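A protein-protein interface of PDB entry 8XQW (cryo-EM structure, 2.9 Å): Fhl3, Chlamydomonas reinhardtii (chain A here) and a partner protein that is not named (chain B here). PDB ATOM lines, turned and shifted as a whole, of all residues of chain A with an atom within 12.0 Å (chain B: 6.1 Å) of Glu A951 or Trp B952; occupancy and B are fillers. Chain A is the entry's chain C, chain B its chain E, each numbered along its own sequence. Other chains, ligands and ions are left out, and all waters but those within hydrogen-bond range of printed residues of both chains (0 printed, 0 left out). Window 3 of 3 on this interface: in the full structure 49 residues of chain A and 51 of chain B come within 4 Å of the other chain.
OE1 of Glu A951 lies within hydrogen-bond range of NE1 of Trp B952, 3.0 Å away.
The side-chain hydroxyl (OG) of Ser A949 lies within hydrogen-bond range of the side-chain amide oxygen (OE1) of Gln A952, 3.2 Å away.
The side-chain carboxylate (OE2) of Glu A951 is in salt-bridge range of the guanidinium group (NH2) of Arg A954, 3.6 Å away.
Ser A949 touches Asp B857 (CA to OD1, 3.8 Å).
Ser A949 touches His B861.
Thr A950 touches Asp B857 (OG1 to OD2, 3.6 Å).
CZ2 of Trp B952 touches CG2 of Thr A950 (3.9 Å).
His B861 touches Glu A951 (NE2 to CB, 3.9 Å).
Glu A951 touches Ile B950 (CG to CG1, 3.9 Å).
His B861 touches Gln A952 (CD2 to OE1, 3.9 Å).
Gln A952 touches Phe B938 (CG to CE2, 3.8 Å).
Trp B952 touches Arg A954.
Printed residues of chain B within 4 Å of Glu A951: His B861 (3.9 Å), Ile B950 (3.9 Å) and Trp B952 (3.0 Å).
Of the printed residues of chain A, Trp B952 touches Thr A950, Glu A951 and Arg A954.
No residue of chain A comes within 4 Å of Gly B949.
Of chain A, only Glu A951 comes within 4 Å of Ile B950.
No residue of chain A comes within 4 Å of Leu B953.
No residue of chain A comes within 4 Å of Asp B954.
No residue of chain A comes within 4 Å of Tyr B957.
Printed residues of chain B within 4 Å of Thr A950: Asp B857 (3.6 Å) and Trp B952 (3.9 Å).
Printed residues of chain A within 4 Å of Phe B938: Gln A952.
Printed residues of chain B within 4 Å of Arg A954: Trp B952.
Of the printed residues of chain B, Gln A952 touches His B861 and Phe B938.
Val A960 touches none of the printed residues of chain B.
The nearest residue of chain B that does not touch Glu A951 is Phe B938 (4.2 Å).
Hydrophobic or aromatic side chains of chain B that line the printed part of chain A: His B861, Phe B938, Ile B950 and Trp B952.
Among the printed residues, 10 pairs touch across the chains.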
ATOM      1  N   ILE A 899     -26.870  17.795 -15.108  1.00  0.00           N
ATOM      2  CA  ILE A 899     -25.831  16.911 -15.623  1.00  0.00           C
ATOM      3  C   ILE A 899     -24.868  16.500 -14.530  1.00  0.00           C
ATOM      4  O   ILE A 899     -24.552  15.321 -14.384  1.00  0.00           O
ATOM      5  CB  ILE A 899     -25.091  17.585 -16.788  1.00  0.00           C
ATOM      6  CG1 ILE A 899     -26.056  17.893 -17.919  1.00  0.00           C
ATOM      7  CG2 ILE A 899     -23.997  16.704 -17.285  1.00  0.00           C
ATOM      8  CD1 ILE A 899     -26.432  16.713 -18.719  1.00  0.00           C
ATOM      9  N   MET A 900     -24.400  17.455 -13.744  1.00  0.00           N
ATOM     10  CA  MET A 900     -23.367  17.206 -12.762  1.00  0.00           C
ATOM     11  C   MET A 900     -23.900  16.950 -11.367  1.00  0.00           C
ATOM     12  O   MET A 900     -23.107  16.705 -10.460  1.00  0.00           O
ATOM     13  CB  MET A 900     -22.398  18.384 -12.717  1.00  0.00           C
ATOM     14  CG  MET A 900     -21.808  18.738 -14.046  1.00  0.00           C
ATOM     15  SD  MET A 900     -20.339  19.739 -13.864  1.00  0.00           S
ATOM     16  CE  MET A 900     -20.408  20.682 -15.371  1.00  0.00           C
ATOM     17  N   ARG A 907     -24.056  10.364 -21.323  1.00  0.00           N
ATOM     18  CA  ARG A 907     -22.712   9.811 -21.254  1.00  0.00           C
ATOM     19  C   ARG A 907     -22.084   9.986 -19.884  1.00  0.00           C
ATOM     20  O   ARG A 907     -21.139   9.271 -19.549  1.00  0.00           O
ATOM     21  CB  ARG A 907     -21.819  10.453 -22.307  1.00  0.00           C
ATOM     22  CG  ARG A 907     -22.228  10.143 -23.717  1.00  0.00           C
ATOM     23  CD  ARG A 907     -22.052  11.353 -24.605  1.00  0.00           C
ATOM     24  NE  ARG A 907     -20.662  11.544 -24.997  1.00  0.00           N
ATOM     25  CZ  ARG A 907     -20.135  12.719 -25.324  1.00  0.00           C
ATOM     26  NH1 ARG A 907     -20.881  13.813 -25.296  1.00  0.00           N
ATOM     27  NH2 ARG A 907     -18.860  12.799 -25.672  1.00  0.00           N
ATOM     28  N   THR A 908     -22.581  10.919 -19.084  1.00  0.00           N
ATOM     29  CA  THR A 908     -22.027  11.122 -17.755  1.00  0.00           C
ATOM     30  C   THR A 908     -22.606  10.150 -16.739  1.00  0.00           C
ATOM     31  O   THR A 908     -21.906   9.743 -15.812  1.00  0.00           O
ATOM     32  CB  THR A 908     -22.273  12.556 -17.307  1.00  0.00           C
ATOM     33  OG1 THR A 908     -21.942  13.440 -18.377  1.00  0.00           O
ATOM     34  CG2 THR A 908     -21.415  12.891 -16.123  1.00  0.00           C
ATOM     35  N   GLY A 909     -23.867   9.773 -16.889  1.00  0.00           N
ATOM     36  CA  GLY A 909     -24.467   8.781 -16.036  1.00  0.00           C
ATOM     37  C   GLY A 909     -24.706   9.293 -14.637  1.00  0.00           C
ATOM     38  O   GLY A 909     -24.504  10.469 -14.340  1.00  0.00           O
ATOM     39  N   ILE A 911     -23.598   9.992 -11.391  1.00  0.00           N
ATOM     40  CA  ILE A 911     -22.506  10.232 -10.458  1.00  0.00           C
ATOM     41  C   ILE A 911     -22.487  11.709 -10.098  1.00  0.00           C
ATOM     42  O   ILE A 911     -22.800  12.573 -10.918  1.00  0.00           O
ATOM     43  CB  ILE A 911     -21.155   9.772 -11.037  1.00  0.00           C
ATOM     44  CG1 ILE A 911     -20.048   9.930 -10.001  1.00  0.00           C
ATOM     45  CG2 ILE A 911     -20.830  10.528 -12.298  1.00  0.00           C
ATOM     46  CD1 ILE A 911     -18.676   9.731 -10.552  1.00  0.00           C
ATOM     47  N   LEU A 913     -20.720  15.196  -8.950  1.00  0.00           N
ATOM     48  CA  LEU A 913     -19.453  15.818  -9.291  1.00  0.00           C
ATOM     49  C   LEU A 913     -19.182  17.131  -8.584  1.00  0.00           C
ATOM     50  O   LEU A 913     -18.031  17.401  -8.256  1.00  0.00           O
ATOM     51  CB  LEU A 913     -19.378  16.049 -10.802  1.00  0.00           C
ATOM     52  CG  LEU A 913     -19.575  14.788 -11.627  1.00  0.00           C
ATOM     53  CD1 LEU A 913     -19.845  15.135 -13.063  1.00  0.00           C
ATOM     54  CD2 LEU A 913     -18.347  13.932 -11.525  1.00  0.00           C
ATOM     55  N   THR A 946     -14.972  21.494  -8.538  1.00  0.00           N
ATOM     56  CA  THR A 946     -14.904  20.155  -9.081  1.00  0.00           C
ATOM     57  C   THR A 946     -13.457  19.711  -9.103  1.00  0.00           C
ATOM     58  O   THR A 946     -12.548  20.531  -9.208  1.00  0.00           O
ATOM     59  CB  THR A 946     -15.472  20.109 -10.486  1.00  0.00           C
ATOM     60  OG1 THR A 946     -16.534  21.055 -10.588  1.00  0.00           O
ATOM     61  CG2 THR A 946     -16.035  18.760 -10.745  1.00  0.00           C
ATOM     62  N   ASP A 947     -13.248  18.405  -9.009  1.00  0.00           N
ATOM     63  CA  ASP A 947     -11.917  17.841  -9.174  1.00  0.00           C
ATOM     64  C   ASP A 947     -11.923  16.667 -10.137  1.00  0.00           C
ATOM     65  O   ASP A 947     -11.056  15.799 -10.054  1.00  0.00           O
ATOM     66  CB  ASP A 947     -11.340  17.422  -7.829  1.00  0.00           C
ATOM     67  CG  ASP A 947     -12.346  16.715  -6.977  1.00  0.00           C
ATOM     68  OD1 ASP A 947     -13.439  16.417  -7.499  1.00  0.00           O
ATOM     69  OD2 ASP A 947     -12.056  16.459  -5.792  1.00  0.00           O
ATOM     70  N   MET A 948     -12.886  16.619 -11.043  1.00  0.00           N
ATOM     71  CA  MET A 948     -12.865  15.583 -12.051  1.00  0.00           C
ATOM     72  C   MET A 948     -11.753  15.863 -13.047  1.00  0.00           C
ATOM     73  O   MET A 948     -11.365  17.007 -13.272  1.00  0.00           O
ATOM     74  CB  MET A 948     -14.208  15.499 -12.764  1.00  0.00           C
ATOM     75  CG  MET A 948     -14.710  16.812 -13.288  1.00  0.00           C
ATOM     76  SD  MET A 948     -16.244  16.606 -14.189  1.00  0.00           S
ATOM     77  CE  MET A 948     -16.871  18.272 -14.170  1.00  0.00           C
ATOM     78  N   SER A 949     -11.236  14.799 -13.642  1.00  0.00           N
ATOM     79  CA  SER A 949     -10.171  14.940 -14.613  1.00  0.00           C
ATOM     80  C   SER A 949     -10.625  15.794 -15.788  1.00  0.00           C
ATOM     81  O   SER A 949     -11.804  16.090 -15.953  1.00  0.00           O
ATOM     82  CB  SER A 949      -9.727  13.574 -15.099  1.00  0.00           C
ATOM     83  OG  SER A 949     -10.828  12.696 -15.100  1.00  0.00           O
ATOM     84  N   THR A 950      -9.661  16.204 -16.606  1.00  0.00           N
ATOM     85  CA  THR A 950      -9.974  17.078 -17.728  1.00  0.00           C
ATOM     86  C   THR A 950     -10.750  16.336 -18.804  1.00  0.00           C
ATOM     87  O   THR A 950     -11.604  16.920 -19.480  1.00  0.00           O
ATOM     88  CB  THR A 950      -8.689  17.663 -18.297  1.00  0.00           C
ATOM     89  OG1 THR A 950      -7.995  18.363 -17.265  1.00  0.00           O
ATOM     90  CG2 THR A 950      -8.987  18.622 -19.410  1.00  0.00           C
ATOM     91  N   GLU A 951     -10.486  15.043 -18.967  1.00  0.00           N
ATOM     92  CA  GLU A 951     -11.183  14.287 -19.994  1.00  0.00           C
ATOM     93  C   GLU A 951     -12.634  14.014 -19.635  1.00  0.00           C
ATOM     94  O   GLU A 951     -13.434  13.724 -20.525  1.00  0.00           O
ATOM     95  CB  GLU A 951     -10.453  12.981 -20.264  1.00  0.00           C
ATOM     96  CG  GLU A 951     -11.039  12.153 -21.388  1.00  0.00           C
ATOM     97  CD  GLU A 951     -11.453  12.976 -22.590  1.00  0.00           C
ATOM     98  OE1 GLU A 951     -10.732  13.915 -22.969  1.00  0.00           O
ATOM     99  OE2 GLU A 951     -12.511  12.678 -23.170  1.00  0.00           O
ATOM    100  N   GLN A 952     -13.003  14.108 -18.366  1.00  0.00           N
ATOM    101  CA  GLN A 952     -14.413  14.006 -18.028  1.00  0.00           C
ATOM    102  C   GLN A 952     -15.070  15.374 -18.003  1.00  0.00           C
ATOM    103  O   GLN A 952     -16.264  15.497 -18.283  1.00  0.00           O
ATOM    104  CB  GLN A 952     -14.565  13.297 -16.694  1.00  0.00           C
ATOM    105  CG  GLN A 952     -13.674  12.092 -16.619  1.00  0.00           C
ATOM    106  CD  GLN A 952     -13.828  11.320 -15.345  1.00  0.00           C
ATOM    107  OE1 GLN A 952     -13.032  10.436 -15.053  1.00  0.00           O
ATOM    108  NE2 GLN A 952     -14.850  11.649 -14.575  1.00  0.00           N
ATOM    109  N   ALA A 953     -14.301  16.412 -17.689  1.00  0.00           N
ATOM    110  CA  ALA A 953     -14.826  17.767 -17.766  1.00  0.00           C
ATOM    111  C   ALA A 953     -15.186  18.136 -19.194  1.00  0.00           C
ATOM    112  O   ALA A 953     -16.189  18.813 -19.429  1.00  0.00           O
ATOM    113  CB  ALA A 953     -13.811  18.749 -17.202  1.00  0.00           C
ATOM    114  N   ARG A 954     -14.377  17.706 -20.161  1.00  0.00           N
ATOM    115  CA  ARG A 954     -14.712  17.941 -21.561  1.00  0.00           C
ATOM    116  C   ARG A 954     -16.085  17.385 -21.899  1.00  0.00           C
ATOM    117  O   ARG A 954     -16.926  18.078 -22.478  1.00  0.00           O
ATOM    118  CB  ARG A 954     -13.662  17.304 -22.459  1.00  0.00           C
ATOM    119  CG  ARG A 954     -12.499  18.189 -22.775  1.00  0.00           C
ATOM    120  CD  ARG A 954     -12.205  18.180 -24.249  1.00  0.00           C
ATOM    121  NE  ARG A 954     -12.024  16.835 -24.766  1.00  0.00           N
ATOM    122  CZ  ARG A 954     -12.930  16.180 -25.476  1.00  0.00           C
ATOM    123  NH1 ARG A 954     -14.092  16.746 -25.748  1.00  0.00           N
ATOM    124  NH2 ARG A 954     -12.681  14.957 -25.909  1.00  0.00           N
ATOM    125  N   VAL A 955     -16.329  16.128 -21.540  1.00  0.00           N
ATOM    126  CA  VAL A 955     -17.591  15.483 -21.871  1.00  0.00           C
ATOM    127  C   VAL A 955     -18.753  16.151 -21.147  1.00  0.00           C
ATOM    128  O   VAL A 955     -19.803  16.424 -21.748  1.00  0.00           O
ATOM    129  CB  VAL A 955     -17.499  13.988 -21.543  1.00  0.00           C
ATOM    130  CG1 VAL A 955     -18.854  13.365 -21.587  1.00  0.00           C
ATOM    131  CG2 VAL A 955     -16.588  13.311 -22.517  1.00  0.00           C
ATOM    132  N   ALA A 956     -18.595  16.428 -19.854  1.00  0.00           N
ATOM    133  CA  ALA A 956     -19.670  17.062 -19.106  1.00  0.00           C
ATOM    134  C   ALA A 956     -20.048  18.409 -19.705  1.00  0.00           C
ATOM    135  O   ALA A 956     -21.236  18.720 -19.861  1.00  0.00           O
ATOM    136  CB  ALA A 956     -19.269  17.223 -17.649  1.00  0.00           C
ATOM    137  N   LEU A 957     -19.059  19.226 -20.056  1.00  0.00           N
ATOM    138  CA  LEU A 957     -19.390  20.526 -20.615  1.00  0.00           C
ATOM    139  C   LEU A 957     -19.986  20.404 -22.006  1.00  0.00           C
ATOM    140  O   LEU A 957     -20.837  21.216 -22.378  1.00  0.00           O
ATOM    141  CB  LEU A 957     -18.165  21.424 -20.641  1.00  0.00           C
ATOM    142  CG  LEU A 957     -17.723  21.975 -19.292  1.00  0.00           C
ATOM    143  CD1 LEU A 957     -17.027  23.291 -19.473  1.00  0.00           C
ATOM    144  CD2 LEU A 957     -18.892  22.140 -18.374  1.00  0.00           C
ATOM    145  N   ALA A 958     -19.571  19.414 -22.790  1.00  0.00           N
ATOM    146  CA  ALA A 958     -20.222  19.216 -24.079  1.00  0.00           C
ATOM    147  C   ALA A 958     -21.700  18.908 -23.899  1.00  0.00           C
ATOM    148  O   ALA A 958     -22.547  19.406 -24.652  1.00  0.00           O
ATOM    149  CB  ALA A 958     -19.532  18.101 -24.853  1.00  0.00           C
ATOM    150  N   GLU A 959     -22.036  18.110 -22.888  1.00  0.00           N
ATOM    151  CA  GLU A 959     -23.441  17.793 -22.652  1.00  0.00           C
ATOM    152  C   GLU A 959     -24.229  19.019 -22.217  1.00  0.00           C
ATOM    153  O   GLU A 959     -25.352  19.243 -22.691  1.00  0.00           O
ATOM    154  CB  GLU A 959     -23.557  16.700 -21.609  1.00  0.00           C
ATOM    155  CG  GLU A 959     -22.753  15.494 -21.946  1.00  0.00           C
ATOM    156  CD  GLU A 959     -23.395  14.238 -21.454  1.00  0.00           C
ATOM    157  OE1 GLU A 959     -24.392  13.810 -22.063  1.00  0.00           O
ATOM    158  OE2 GLU A 959     -22.910  13.682 -20.451  1.00  0.00           O
ATOM    159  N   VAL A 960     -23.669  19.817 -21.311  1.00  0.00           N
ATOM    160  CA  VAL A 960     -24.334  21.056 -20.919  1.00  0.00           C
ATOM    161  C   VAL A 960     -24.591  21.936 -22.132  1.00  0.00           C
ATOM    162  O   VAL A 960     -25.681  22.500 -22.297  1.00  0.00           O
ATOM    163  CB  VAL A 960     -23.499  21.802 -19.870  1.00  0.00           C
ATOM    164  CG1 VAL A 960     -24.123  23.122 -19.582  1.00  0.00           C
ATOM    165  CG2 VAL A 960     -23.386  20.994 -18.613  1.00  0.00           C
ATOM    166  N   ASP B 857      -3.703  13.559 -12.162  1.00  0.00           N
ATOM    167  CA  ASP B 857      -4.663  13.911 -13.204  1.00  0.00           C
ATOM    168  C   ASP B 857      -4.539  13.058 -14.458  1.00  0.00           C
ATOM    169  O   ASP B 857      -5.276  13.265 -15.423  1.00  0.00           O
ATOM    170  CB  ASP B 857      -4.548  15.379 -13.580  1.00  0.00           C
ATOM    171  CG  ASP B 857      -5.847  15.935 -14.114  1.00  0.00           C
ATOM    172  OD1 ASP B 857      -6.790  16.123 -13.319  1.00  0.00           O
ATOM    173  OD2 ASP B 857      -5.929  16.173 -15.335  1.00  0.00           O
ATOM    174  N   HIS B 861      -7.505  10.139 -13.422  1.00  0.00           N
ATOM    175  CA  HIS B 861      -8.429   9.681 -14.450  1.00  0.00           C
ATOM    176  C   HIS B 861      -8.789   8.218 -14.245  1.00  0.00           C
ATOM    177  O   HIS B 861      -9.969   7.863 -14.177  1.00  0.00           O
ATOM    178  CB  HIS B 861      -7.807   9.895 -15.824  1.00  0.00           C
ATOM    179  CG  HIS B 861      -8.730   9.613 -16.961  1.00  0.00           C
ATOM    180  ND1 HIS B 861      -8.458   8.661 -17.915  1.00  0.00           N
ATOM    181  CD2 HIS B 861      -9.908  10.170 -17.313  1.00  0.00           C
ATOM    182  CE1 HIS B 861      -9.437   8.633 -18.796  1.00  0.00           C
ATOM    183  NE2 HIS B 861     -10.331   9.539 -18.454  1.00  0.00           N
ATOM    184  N   PHE B 938     -14.270   5.049 -19.497  1.00  0.00           N
ATOM    185  CA  PHE B 938     -13.235   5.511 -20.410  1.00  0.00           C
ATOM    186  C   PHE B 938     -12.143   4.474 -20.611  1.00  0.00           C
ATOM    187  O   PHE B 938     -11.795   4.146 -21.748  1.00  0.00           O
ATOM    188  CB  PHE B 938     -12.638   6.815 -19.897  1.00  0.00           C
ATOM    189  CG  PHE B 938     -13.629   7.922 -19.773  1.00  0.00           C
ATOM    190  CD1 PHE B 938     -13.922   8.722 -20.848  1.00  0.00           C
ATOM    191  CD2 PHE B 938     -14.259   8.167 -18.581  1.00  0.00           C
ATOM    192  CE1 PHE B 938     -14.824   9.740 -20.733  1.00  0.00           C
ATOM    193  CE2 PHE B 938     -15.162   9.185 -18.471  1.00  0.00           C
ATOM    194  CZ  PHE B 938     -15.445   9.970 -19.545  1.00  0.00           C
ATOM    195  N   GLY B 949      -7.370   6.165 -24.047  1.00  0.00           N
ATOM    196  CA  GLY B 949      -8.496   6.692 -24.777  1.00  0.00           C
ATOM    197  C   GLY B 949      -8.630   8.192 -24.762  1.00  0.00           C
ATOM    198  O   GLY B 949      -9.689   8.702 -25.127  1.00  0.00           O
ATOM    199  N   ILE B 950      -7.602   8.920 -24.341  1.00  0.00           N
ATOM    200  CA  ILE B 950      -7.601  10.373 -24.415  1.00  0.00           C
ATOM    201  C   ILE B 950      -6.962  10.758 -25.737  1.00  0.00           C
ATOM    202  O   ILE B 950      -5.829  10.375 -26.023  1.00  0.00           O
ATOM    203  CB  ILE B 950      -6.852  11.003 -23.244  1.00  0.00           C
ATOM    204  CG1 ILE B 950      -7.473  10.592 -21.932  1.00  0.00           C
ATOM    205  CG2 ILE B 950      -6.940  12.476 -23.341  1.00  0.00           C
ATOM    206  CD1 ILE B 950      -6.753  11.152 -20.765  1.00  0.00           C
ATOM    207  N   GLU B 951      -7.686  11.518 -26.548  1.00  0.00           N
ATOM    208  CA  GLU B 951      -7.176  11.856 -27.867  1.00  0.00           C
ATOM    209  C   GLU B 951      -6.048  12.875 -27.793  1.00  0.00           C
ATOM    210  O   GLU B 951      -5.110  12.821 -28.592  1.00  0.00           O
ATOM    211  CB  GLU B 951      -8.314  12.382 -28.735  1.00  0.00           C
ATOM    212  CG  GLU B 951      -7.871  13.100 -29.981  1.00  0.00           C
ATOM    213  CD  GLU B 951      -8.987  13.237 -30.993  1.00  0.00           C
ATOM    214  OE1 GLU B 951      -8.910  12.586 -32.057  1.00  0.00           O
ATOM    215  OE2 GLU B 951      -9.945  13.991 -30.724  1.00  0.00           O
ATOM    216  N   TRP B 952      -6.106  13.785 -26.832  1.00  0.00           N
ATOM    217  CA  TRP B 952      -5.175  14.895 -26.768  1.00  0.00           C
ATOM    218  C   TRP B 952      -4.009  14.663 -25.830  1.00  0.00           C
ATOM    219  O   TRP B 952      -3.265  15.603 -25.564  1.00  0.00           O
ATOM    220  CB  TRP B 952      -5.907  16.156 -26.338  1.00  0.00           C
ATOM    221  CG  TRP B 952      -6.688  15.989 -25.098  1.00  0.00           C
ATOM    222  CD1 TRP B 952      -8.000  15.685 -25.002  1.00  0.00           C
ATOM    223  CD2 TRP B 952      -6.209  16.128 -23.764  1.00  0.00           C
ATOM    224  NE1 TRP B 952      -8.376  15.626 -23.691  1.00  0.00           N
ATOM    225  CE2 TRP B 952      -7.288  15.895 -22.910  1.00  0.00           C
ATOM    226  CE3 TRP B 952      -4.970  16.430 -23.210  1.00  0.00           C
ATOM    227  CZ2 TRP B 952      -7.164  15.944 -21.539  1.00  0.00           C
ATOM    228  CZ3 TRP B 952      -4.853  16.479 -21.849  1.00  0.00           C
ATOM    229  CH2 TRP B 952      -5.939  16.237 -21.030  1.00  0.00           C
ATOM    230  N   LEU B 953      -3.831  13.454 -25.311  1.00  0.00           N
ATOM    231  CA  LEU B 953      -2.813  13.260 -24.289  1.00  0.00           C
ATOM    232  C   LEU B 953      -1.416  13.375 -24.859  1.00  0.00           C
ATOM    233  O   LEU B 953      -0.491  13.768 -24.147  1.00  0.00           O
ATOM    234  CB  LEU B 953      -2.981  11.909 -23.620  1.00  0.00           C
ATOM    235  CG  LEU B 953      -2.363  11.868 -22.241  1.00  0.00           C
ATOM    236  CD1 LEU B 953      -3.019  12.895 -21.389  1.00  0.00           C
ATOM    237  CD2 LEU B 953      -2.542  10.519 -21.643  1.00  0.00           C
ATOM    238  N   ASP B 954      -1.235  13.035 -26.124  1.00  0.00           N
ATOM    239  CA  ASP B 954       0.093  13.081 -26.708  1.00  0.00           C
ATOM    240  C   ASP B 954       0.475  14.462 -27.207  1.00  0.00           C
ATOM    241  O   ASP B 954       1.616  14.652 -27.630  1.00  0.00           O
ATOM    242  CB  ASP B 954       0.180  12.072 -27.839  1.00  0.00           C
ATOM    243  CG  ASP B 954       0.152  10.654 -27.338  1.00  0.00           C
ATOM    244  OD1 ASP B 954       0.965  10.330 -26.450  1.00  0.00           O
ATOM    245  OD2 ASP B 954      -0.684   9.866 -27.820  1.00  0.00           O
ATOM    246  N   ASP B 955      -0.440  15.419 -27.178  1.00  0.00           N
ATOM    247  CA  ASP B 955      -0.112  16.805 -27.463  1.00  0.00           C
ATOM    248  C   ASP B 955       0.132  17.614 -26.207  1.00  0.00           C
ATOM    249  O   ASP B 955       0.430  18.803 -26.310  1.00  0.00           O
ATOM    250  CB  ASP B 955      -1.227  17.478 -28.257  1.00  0.00           C
ATOM    251  CG  ASP B 955      -1.440  16.853 -29.605  1.00  0.00           C
ATOM    252  OD1 ASP B 955      -0.454  16.420 -30.221  1.00  0.00           O
ATOM    253  OD2 ASP B 955      -2.599  16.799 -30.061  1.00  0.00           O
ATOM    254  N   ALA B 956      -0.007  17.015 -25.038  1.00  0.00           N
ATOM    255  CA  ALA B 956       0.158  17.725 -23.786  1.00  0.00           C
ATOM    256  C   ALA B 956       1.248  17.165 -22.903  1.00  0.00           C
ATOM    257  O   ALA B 956       1.894  17.933 -22.199  1.00  0.00           O
ATOM    258  CB  ALA B 956      -1.149  17.719 -22.993  1.00  0.00           C
ATOM    259  N   TYR B 957       1.473  15.858 -22.923  1.00  0.00           N
ATOM    260  CA  TYR B 957       2.411  15.208 -22.037  1.00  0.00           C
ATOM    261  C   TYR B 957       3.510  14.535 -22.840  1.00  0.00           C
ATOM    262  O   TYR B 957       3.212  13.857 -23.831  1.00  0.00           O
ATOM    263  CB  TYR B 957       1.708  14.164 -21.183  1.00  0.00           C
ATOM    264  CG  TYR B 957       0.963  14.733 -20.022  1.00  0.00           C
ATOM    265  CD1 TYR B 957      -0.216  15.410 -20.207  1.00  0.00           C
ATOM    266  CD2 TYR B 957       1.438  14.598 -18.748  1.00  0.00           C
ATOM    267  CE1 TYR B 957      -0.895  15.937 -19.156  1.00  0.00           C
ATOM    268  CE2 TYR B 957       0.762  15.118 -17.693  1.00  0.00           C
ATOM    269  CZ  TYR B 957      -0.403  15.785 -17.901  1.00  0.00           C
ATOM    270  OH  TYR B 957      -1.079  16.309 -16.835  1.00  0.00           O
